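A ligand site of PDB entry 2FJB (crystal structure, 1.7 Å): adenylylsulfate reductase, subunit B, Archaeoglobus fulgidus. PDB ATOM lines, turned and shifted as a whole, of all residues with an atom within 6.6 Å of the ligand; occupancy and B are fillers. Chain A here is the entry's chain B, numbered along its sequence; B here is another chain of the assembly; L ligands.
The side-chain sulfur (SD) of Met 30 sits close to a sulfur (S3) of the ligand (3.7 Å).
Residues that only touch the ligand: Pro 26, Leu 29, Glu 49 and Ser 52.
Hydrophobic or aromatic side chains that line the ligand: Pro 26, Leu 29 and Met 30.
Within 4 Å of the ligand: Ser 3, Cys 25, Pro 26, Leu 29, Met 30, Asn 41, Cys 47, Trp 48, Glu 49, Cys 50, Tyr 51, Ser 52 and Cys 53.
Along chain A the residues within 4 Å of the ligand span positions 3 to 53.
The nearest printed residue that does not touch the ligand is Phe 238 of chain B (4.3 Å).
A sulfur (S4) of the ligand sits close to the backbone NH (N) of Trp 48, 3.6 Å away.
S3 of the ligand lies close to OG of Ser 3 (3.2 Å).
A sulfur (S1) of the ligand sits close to the backbone NH (N) of Cys 50, at 3.4 Å.
N of Cys 53 lies close to S2 of the ligand (3.4 Å).
ND2 of Asn 41 sits close to S3 of the ligand (3.6 Å).
The side-chain sulfur (SG) of Cys 25 binds an iron atom (FE1) of the ligand, at 2.4 Å.
The side-chain sulfur (SG) of Cys 50 is bound to an iron atom (FE3) of the ligand, at 2.4 Å.
SG of Cys 47 binds FE2 of the ligand, at 2.4 Å.
An iron atom (FE4) of the ligand is bound by the side-chain sulfur of Cys 53.
The backbone NH (N) of Tyr 51 lies close to a sulfur (S1) of the ligand.
The side-chain hydroxyl (OG) of Ser 3 lies within hydrogen-bond range of the side-chain sulfur (SD) of Met 30, 3.5 Å away.
The side-chain sulfur of Cys 47 sits close to the backbone NH of Ser 3.
SG of Cys 25 lies close to N of Asp 28.
The side-chain sulfur of Cys 25 lies close to the backbone NH of Asn 27 (3.4 Å).
The side-chain sulfur (SG) of Cys 47 lies close to the backbone NH (N) of Glu 49 (3.4 Å).
The side-chain hydroxyl (OG) of Ser 3 sits at hydrogen-bond distance from the side-chain amide nitrogen (ND2) of Asn 41 (3.1 Å).
The side-chain hydroxyl (OG) of Ser 52 sits close to the side-chain sulfur (SG) of Cys 50, 3.2 Å away.
The backbone NH of Leu 29 sits close to the side-chain sulfur of Cys 25.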
ATOM      1  N   PRO A   2     -11.117  36.204  22.184  1.00  0.00           N
ATOM      2  CA  PRO A   2     -11.195  35.160  21.163  1.00  0.00           C
ATOM      3  C   PRO A   2     -10.141  35.349  20.077  1.00  0.00           C
ATOM      4  O   PRO A   2      -9.592  36.427  19.916  1.00  0.00           O
ATOM      5  CB  PRO A   2     -12.615  35.318  20.626  1.00  0.00           C
ATOM      6  CG  PRO A   2     -13.372  35.749  21.842  1.00  0.00           C
ATOM      7  CD  PRO A   2     -12.451  36.775  22.458  1.00  0.00           C
ATOM      8  N   SER A   3      -9.865  34.288  19.330  1.00  0.00           N
ATOM      9  CA  SER A   3      -8.871  34.363  18.261  1.00  0.00           C
ATOM     10  C   SER A   3      -9.426  35.081  17.041  1.00  0.00           C
ATOM     11  O   SER A   3     -10.643  35.157  16.849  1.00  0.00           O
ATOM     12  CB  SER A   3      -8.431  32.963  17.841  1.00  0.00           C
ATOM     13  OG  SER A   3      -9.486  32.292  17.190  1.00  0.00           O
ATOM     14  N   CYS A  21      -4.928  25.782  11.528  1.00  0.00           N
ATOM     15  CA  CYS A  21      -5.894  26.273  12.499  1.00  0.00           C
ATOM     16  C   CYS A  21      -7.165  25.428  12.549  1.00  0.00           C
ATOM     17  O   CYS A  21      -7.651  25.097  13.624  1.00  0.00           O
ATOM     18  CB  CYS A  21      -6.243  27.736  12.203  1.00  0.00           C
ATOM     19  SG  CYS A  21      -6.996  28.042  10.585  1.00  0.00           S
ATOM     20  N   ILE A  24      -6.343  21.973  14.270  1.00  0.00           N
ATOM     21  CA  ILE A  24      -6.053  21.946  15.703  1.00  0.00           C
ATOM     22  C   ILE A  24      -7.121  22.362  16.719  1.00  0.00           C
ATOM     23  O   ILE A  24      -7.147  21.831  17.828  1.00  0.00           O
ATOM     24  CB  ILE A  24      -4.770  22.768  15.995  1.00  0.00           C
ATOM     25  CG1 ILE A  24      -4.112  22.274  17.289  1.00  0.00           C
ATOM     26  CG2 ILE A  24      -5.119  24.249  16.110  1.00  0.00           C
ATOM     27  CD1 ILE A  24      -3.453  20.908  17.173  1.00  0.00           C
ATOM     28  N   CYS A  25      -7.990  23.306  16.346  1.00  0.00           N
ATOM     29  CA  CYS A  25      -9.006  23.817  17.263  1.00  0.00           C
ATOM     30  C   CYS A  25      -9.852  22.764  17.996  1.00  0.00           C
ATOM     31  O   CYS A  25     -10.624  22.044  17.375  1.00  0.00           O
ATOM     32  CB  CYS A  25      -9.943  24.783  16.555  1.00  0.00           C
ATOM     33  SG  CYS A  25     -11.170  25.494  17.676  1.00  0.00           S
ATOM     34  N   PRO A  26      -9.711  22.689  19.329  1.00  0.00           N
ATOM     35  CA  PRO A  26     -10.443  21.735  20.168  1.00  0.00           C
ATOM     36  C   PRO A  26     -11.961  21.940  20.185  1.00  0.00           C
ATOM     37  O   PRO A  26     -12.694  21.044  20.622  1.00  0.00           O
ATOM     38  CB  PRO A  26      -9.826  21.939  21.548  1.00  0.00           C
ATOM     39  CG  PRO A  26      -8.471  22.503  21.258  1.00  0.00           C
ATOM     40  CD  PRO A  26      -8.757  23.465  20.142  1.00  0.00           C
ATOM     41  N   ASN A  27     -12.430  23.102  19.735  1.00  0.00           N
ATOM     42  CA  ASN A  27     -13.871  23.362  19.736  1.00  0.00           C
ATOM     43  C   ASN A  27     -14.455  23.577  18.331  1.00  0.00           C
ATOM     44  O   ASN A  27     -15.572  24.061  18.190  1.00  0.00           O
ATOM     45  CB  ASN A  27     -14.192  24.552  20.649  1.00  0.00           C
ATOM     46  CG  ASN A  27     -15.487  24.353  21.429  1.00  0.00           C
ATOM     47  OD1 ASN A  27     -15.962  23.231  21.595  1.00  0.00           O
ATOM     48  ND2 ASN A  27     -16.050  25.451  21.936  1.00  0.00           N
ATOM     49  N   ASP A  28     -13.690  23.202  17.305  1.00  0.00           N
ATOM     50  CA  ASP A  28     -14.112  23.325  15.912  1.00  0.00           C
ATOM     51  C   ASP A  28     -14.541  24.737  15.501  1.00  0.00           C
ATOM     52  O   ASP A  28     -15.545  24.918  14.801  1.00  0.00           O
ATOM     53  CB  ASP A  28     -15.252  22.327  15.642  1.00  0.00           C
ATOM     54  CG  ASP A  28     -15.651  22.260  14.174  1.00  0.00           C
ATOM     55  OD1 ASP A  28     -14.743  22.207  13.312  1.00  0.00           O
ATOM     56  OD2 ASP A  28     -16.869  22.254  13.873  1.00  0.00           O
ATOM     57  N   LEU A  29     -13.759  25.735  15.898  1.00  0.00           N
ATOM     58  CA  LEU A  29     -14.084  27.121  15.595  1.00  0.00           C
ATOM     59  C   LEU A  29     -13.397  27.665  14.348  1.00  0.00           C
ATOM     60  O   LEU A  29     -13.981  28.457  13.616  1.00  0.00           O
ATOM     61  CB  LEU A  29     -13.722  28.023  16.777  1.00  0.00           C
ATOM     62  CG  LEU A  29     -14.311  27.638  18.138  1.00  0.00           C
ATOM     63  CD1 LEU A  29     -13.959  28.735  19.136  1.00  0.00           C
ATOM     64  CD2 LEU A  29     -15.820  27.447  18.031  1.00  0.00           C
ATOM     65  N   MET A  30     -12.157  27.250  14.106  1.00  0.00           N
ATOM     66  CA  MET A  30     -11.434  27.749  12.943  1.00  0.00           C
ATOM     67  C   MET A  30     -11.848  27.027  11.664  1.00  0.00           C
ATOM     68  O   MET A  30     -11.900  25.797  11.610  1.00  0.00           O
ATOM     69  CB  MET A  30      -9.920  27.596  13.155  1.00  0.00           C
ATOM     70  CG  MET A  30      -9.395  28.321  14.392  1.00  0.00           C
ATOM     71  SD  MET A  30      -9.913  30.066  14.471  1.00  0.00           S
ATOM     72  CE  MET A  30      -9.058  30.743  13.063  1.00  0.00           C
ATOM     73  N   ASN A  41     -12.616  32.713  12.798  1.00  0.00           N
ATOM     74  CA  ASN A  41     -13.217  32.016  13.932  1.00  0.00           C
ATOM     75  C   ASN A  41     -14.721  32.105  13.671  1.00  0.00           C
ATOM     76  O   ASN A  41     -15.282  33.201  13.617  1.00  0.00           O
ATOM     77  CB  ASN A  41     -12.848  32.741  15.228  1.00  0.00           C
ATOM     78  CG  ASN A  41     -13.361  32.032  16.448  1.00  0.00           C
ATOM     79  OD1 ASN A  41     -14.497  31.552  16.471  1.00  0.00           O
ATOM     80  ND2 ASN A  41     -12.541  31.971  17.495  1.00  0.00           N
ATOM     81  N   MET A  46     -17.532  30.895  21.774  1.00  0.00           N
ATOM     82  CA  MET A  46     -17.281  29.514  22.182  1.00  0.00           C
ATOM     83  C   MET A  46     -15.767  29.265  22.186  1.00  0.00           C
ATOM     84  O   MET A  46     -15.310  28.125  22.294  1.00  0.00           O
ATOM     85  CB  MET A  46     -17.977  28.518  21.250  1.00  0.00           C
ATOM     86  CG  MET A  46     -19.492  28.417  21.492  1.00  0.00           C
ATOM     87  SD  MET A  46     -19.929  27.871  23.156  1.00  0.00           S
ATOM     88  CE  MET A  46     -19.412  26.014  23.018  1.00  0.00           C
ATOM     89  N   CYS A  47     -14.993  30.347  22.080  1.00  0.00           N
ATOM     90  CA  CYS A  47     -13.538  30.279  22.086  1.00  0.00           C
ATOM     91  C   CYS A  47     -13.038  30.270  23.523  1.00  0.00           C
ATOM     92  O   CYS A  47     -13.407  31.116  24.327  1.00  0.00           O
ATOM     93  CB  CYS A  47     -12.940  31.474  21.336  1.00  0.00           C
ATOM     94  SG  CYS A  47     -11.124  31.541  21.264  1.00  0.00           S
ATOM     95  N   TRP A  48     -12.183  29.294  23.835  1.00  0.00           N
ATOM     96  CA  TRP A  48     -11.624  29.141  25.177  1.00  0.00           C
ATOM     97  C   TRP A  48     -10.319  29.933  25.321  1.00  0.00           C
ATOM     98  O   TRP A  48      -9.746  30.005  26.400  1.00  0.00           O
ATOM     99  CB  TRP A  48     -11.363  27.659  25.428  1.00  0.00           C
ATOM    100  CG  TRP A  48     -11.366  27.230  26.867  1.00  0.00           C
ATOM    101  CD1 TRP A  48     -12.299  27.549  27.813  1.00  0.00           C
ATOM    102  CD2 TRP A  48     -10.449  26.317  27.493  1.00  0.00           C
ATOM    103  NE1 TRP A  48     -12.030  26.888  28.994  1.00  0.00           N
ATOM    104  CE2 TRP A  48     -10.891  26.126  28.820  1.00  0.00           C
ATOM    105  CE3 TRP A  48      -9.302  25.645  27.058  1.00  0.00           C
ATOM    106  CZ2 TRP A  48     -10.231  25.287  29.719  1.00  0.00           C
ATOM    107  CZ3 TRP A  48      -8.642  24.807  27.957  1.00  0.00           C
ATOM    108  CH2 TRP A  48      -9.114  24.634  29.271  1.00  0.00           C
ATOM    109  N   GLU A  49      -9.881  30.548  24.218  1.00  0.00           N
ATOM    110  CA  GLU A  49      -8.621  31.291  24.189  1.00  0.00           C
ATOM    111  C   GLU A  49      -7.476  30.384  24.639  1.00  0.00           C
ATOM    112  O   GLU A  49      -6.663  30.760  25.489  1.00  0.00           O
ATOM    113  CB  GLU A  49      -8.691  32.568  25.046  1.00  0.00           C
ATOM    114  CG  GLU A  49      -9.527  33.691  24.423  1.00  0.00           C
ATOM    115  CD  GLU A  49      -9.373  35.049  25.113  1.00  0.00           C
ATOM    116  OE1 GLU A  49      -8.750  35.132  26.195  1.00  0.00           O
ATOM    117  OE2 GLU A  49      -9.887  36.055  24.563  1.00  0.00           O
ATOM    118  N   CYS A  50      -7.434  29.184  24.059  1.00  0.00           N
ATOM    119  CA  CYS A  50      -6.397  28.213  24.403  1.00  0.00           C
ATOM    120  C   CYS A  50      -5.114  28.440  23.622  1.00  0.00           C
ATOM    121  O   CYS A  50      -4.085  27.836  23.920  1.00  0.00           O
ATOM    122  CB  CYS A  50      -6.908  26.783  24.161  1.00  0.00           C
ATOM    123  SG  CYS A  50      -7.084  26.300  22.423  1.00  0.00           S
ATOM    124  N   TYR A  51      -5.187  29.303  22.612  1.00  0.00           N
ATOM    125  CA  TYR A  51      -4.052  29.648  21.769  1.00  0.00           C
ATOM    126  C   TYR A  51      -3.468  28.522  20.923  1.00  0.00           C
ATOM    127  O   TYR A  51      -2.361  28.639  20.413  1.00  0.00           O
ATOM    128  CB  TYR A  51      -2.931  30.269  22.615  1.00  0.00           C
ATOM    129  CG  TYR A  51      -3.154  31.730  22.979  1.00  0.00           C
ATOM    130  CD1 TYR A  51      -4.119  32.100  23.912  1.00  0.00           C
ATOM    131  CD2 TYR A  51      -2.404  32.735  22.381  1.00  0.00           C
ATOM    132  CE1 TYR A  51      -4.328  33.435  24.258  1.00  0.00           C
ATOM    133  CE2 TYR A  51      -2.594  34.078  22.719  1.00  0.00           C
ATOM    134  CZ  TYR A  51      -3.557  34.417  23.652  1.00  0.00           C
ATOM    135  OH  TYR A  51      -3.739  35.741  23.991  1.00  0.00           O
ATOM    136  N   SER A  52      -4.208  27.422  20.771  1.00  0.00           N
ATOM    137  CA  SER A  52      -3.702  26.318  19.970  1.00  0.00           C
ATOM    138  C   SER A  52      -3.532  26.744  18.511  1.00  0.00           C
ATOM    139  O   SER A  52      -2.506  26.492  17.891  1.00  0.00           O
ATOM    140  CB  SER A  52      -4.637  25.109  20.047  1.00  0.00           C
ATOM    141  OG  SER A  52      -4.615  24.542  21.350  1.00  0.00           O
ATOM    142  N   CYS A  53      -4.556  27.417  17.982  1.00  0.00           N
ATOM    143  CA  CYS A  53      -4.515  27.876  16.594  1.00  0.00           C
ATOM    144  C   CYS A  53      -3.371  28.878  16.414  1.00  0.00           C
ATOM    145  O   CYS A  53      -2.624  28.804  15.442  1.00  0.00           O
ATOM    146  CB  CYS A  53      -5.846  28.529  16.216  1.00  0.00           C
ATOM    147  SG  CYS A  53      -6.355  29.927  17.263  1.00  0.00           S
ATOM    148  N   VAL A  54      -3.245  29.797  17.370  1.00  0.00           N
ATOM    149  CA  VAL A  54      -2.194  30.818  17.313  1.00  0.00           C
ATOM    150  C   VAL A  54      -0.807  30.179  17.204  1.00  0.00           C
ATOM    151  O   VAL A  54       0.002  30.565  16.359  1.00  0.00           O
ATOM    152  CB  VAL A  54      -2.199  31.694  18.582  1.00  0.00           C
ATOM    153  CG1 VAL A  54      -1.023  32.651  18.565  1.00  0.00           C
ATOM    154  CG2 VAL A  54      -3.511  32.463  18.674  1.00  0.00           C
ATOM    155  N   ILE A  62      -2.498  34.453  13.238  1.00  0.00           N
ATOM    156  CA  ILE A  62      -3.561  34.420  14.230  1.00  0.00           C
ATOM    157  C   ILE A  62      -3.136  35.062  15.551  1.00  0.00           C
ATOM    158  O   ILE A  62      -2.036  34.815  16.049  1.00  0.00           O
ATOM    159  CB  ILE A  62      -4.018  32.972  14.503  1.00  0.00           C
ATOM    160  CG1 ILE A  62      -4.366  32.277  13.188  1.00  0.00           C
ATOM    161  CG2 ILE A  62      -5.245  32.973  15.415  1.00  0.00           C
ATOM    162  CD1 ILE A  62      -4.819  30.836  13.351  1.00  0.00           C
ATOM    163  N   VAL A  64      -4.969  36.865  19.452  1.00  0.00           N
ATOM    164  CA  VAL A  64      -6.117  36.791  20.330  1.00  0.00           C
ATOM    165  C   VAL A  64      -6.420  38.159  20.900  1.00  0.00           C
ATOM    166  O   VAL A  64      -5.511  38.866  21.350  1.00  0.00           O
ATOM    167  CB  VAL A  64      -5.871  35.791  21.484  1.00  0.00           C
ATOM    168  CG1 VAL A  64      -7.006  35.892  22.500  1.00  0.00           C
ATOM    169  CG2 VAL A  64      -5.809  34.371  20.929  1.00  0.00           C
ATOM    170  N   ALA B  67      -5.619  21.430  26.544  1.00  0.00           N
ATOM    171  CA  ALA B  67      -5.298  22.107  25.282  1.00  0.00           C
ATOM    172  C   ALA B  67      -4.220  23.191  25.406  1.00  0.00           C
ATOM    173  O   ALA B  67      -3.384  23.325  24.527  1.00  0.00           O
ATOM    174  CB  ALA B  67      -6.563  22.713  24.688  1.00  0.00           C
ATOM    175  N   ILE B 237     -14.367  23.887  28.075  1.00  0.00           N
ATOM    176  CA  ILE B 237     -15.608  24.204  27.387  1.00  0.00           C
ATOM    177  C   ILE B 237     -15.893  23.112  26.342  1.00  0.00           C
ATOM    178  O   ILE B 237     -17.029  22.940  25.899  1.00  0.00           O
ATOM    179  CB  ILE B 237     -15.480  25.587  26.682  1.00  0.00           C
ATOM    180  CG1 ILE B 237     -16.826  26.004  26.086  1.00  0.00           C
ATOM    181  CG2 ILE B 237     -14.406  25.532  25.601  1.00  0.00           C
ATOM    182  CD1 ILE B 237     -16.824  27.426  25.542  1.00  0.00           C
ATOM    183  N   PHE B 238     -14.855  22.352  26.002  1.00  0.00           N
ATOM    184  CA  PHE B 238     -14.951  21.270  25.020  1.00  0.00           C
ATOM    185  C   PHE B 238     -15.697  20.044  25.551  1.00  0.00           C
ATOM    186  O   PHE B 238     -16.159  19.214  24.772  1.00  0.00           O
ATOM    187  CB  PHE B 238     -13.555  20.828  24.577  1.00  0.00           C
ATOM    188  CG  PHE B 238     -12.575  21.968  24.444  1.00  0.00           C
ATOM    189  CD1 PHE B 238     -11.423  21.987  25.221  1.00  0.00           C
ATOM    190  CD2 PHE B 238     -12.810  23.006  23.560  1.00  0.00           C
ATOM    191  CE1 PHE B 238     -10.516  23.040  25.114  1.00  0.00           C
ATOM    192  CE2 PHE B 238     -11.915  24.065  23.443  1.00  0.00           C
ATOM    193  CZ  PHE B 238     -10.764  24.084  24.230  1.00  0.00           C
HETATM  194 FE1  LIG L   1     -10.020  27.199  18.968  1.00  0.00          FE
HETATM  195 FE2  LIG L   1     -10.156  29.563  20.326  1.00  0.00          FE
HETATM  196 FE3  LIG L   1      -8.413  27.628  20.992  1.00  0.00          FE
HETATM  197 FE4  LIG L   1      -8.090  29.004  18.707  1.00  0.00          FE
HETATM  198  S1  LIG L   1      -7.978  29.925  20.815  1.00  0.00           S
HETATM  199  S2  LIG L   1      -7.791  26.863  19.010  1.00  0.00           S
HETATM  200  S3  LIG L   1     -10.244  29.316  18.109  1.00  0.00           S
HETATM  201  S4  LIG L   1     -10.635  27.496  21.188  1.00  0.00           S
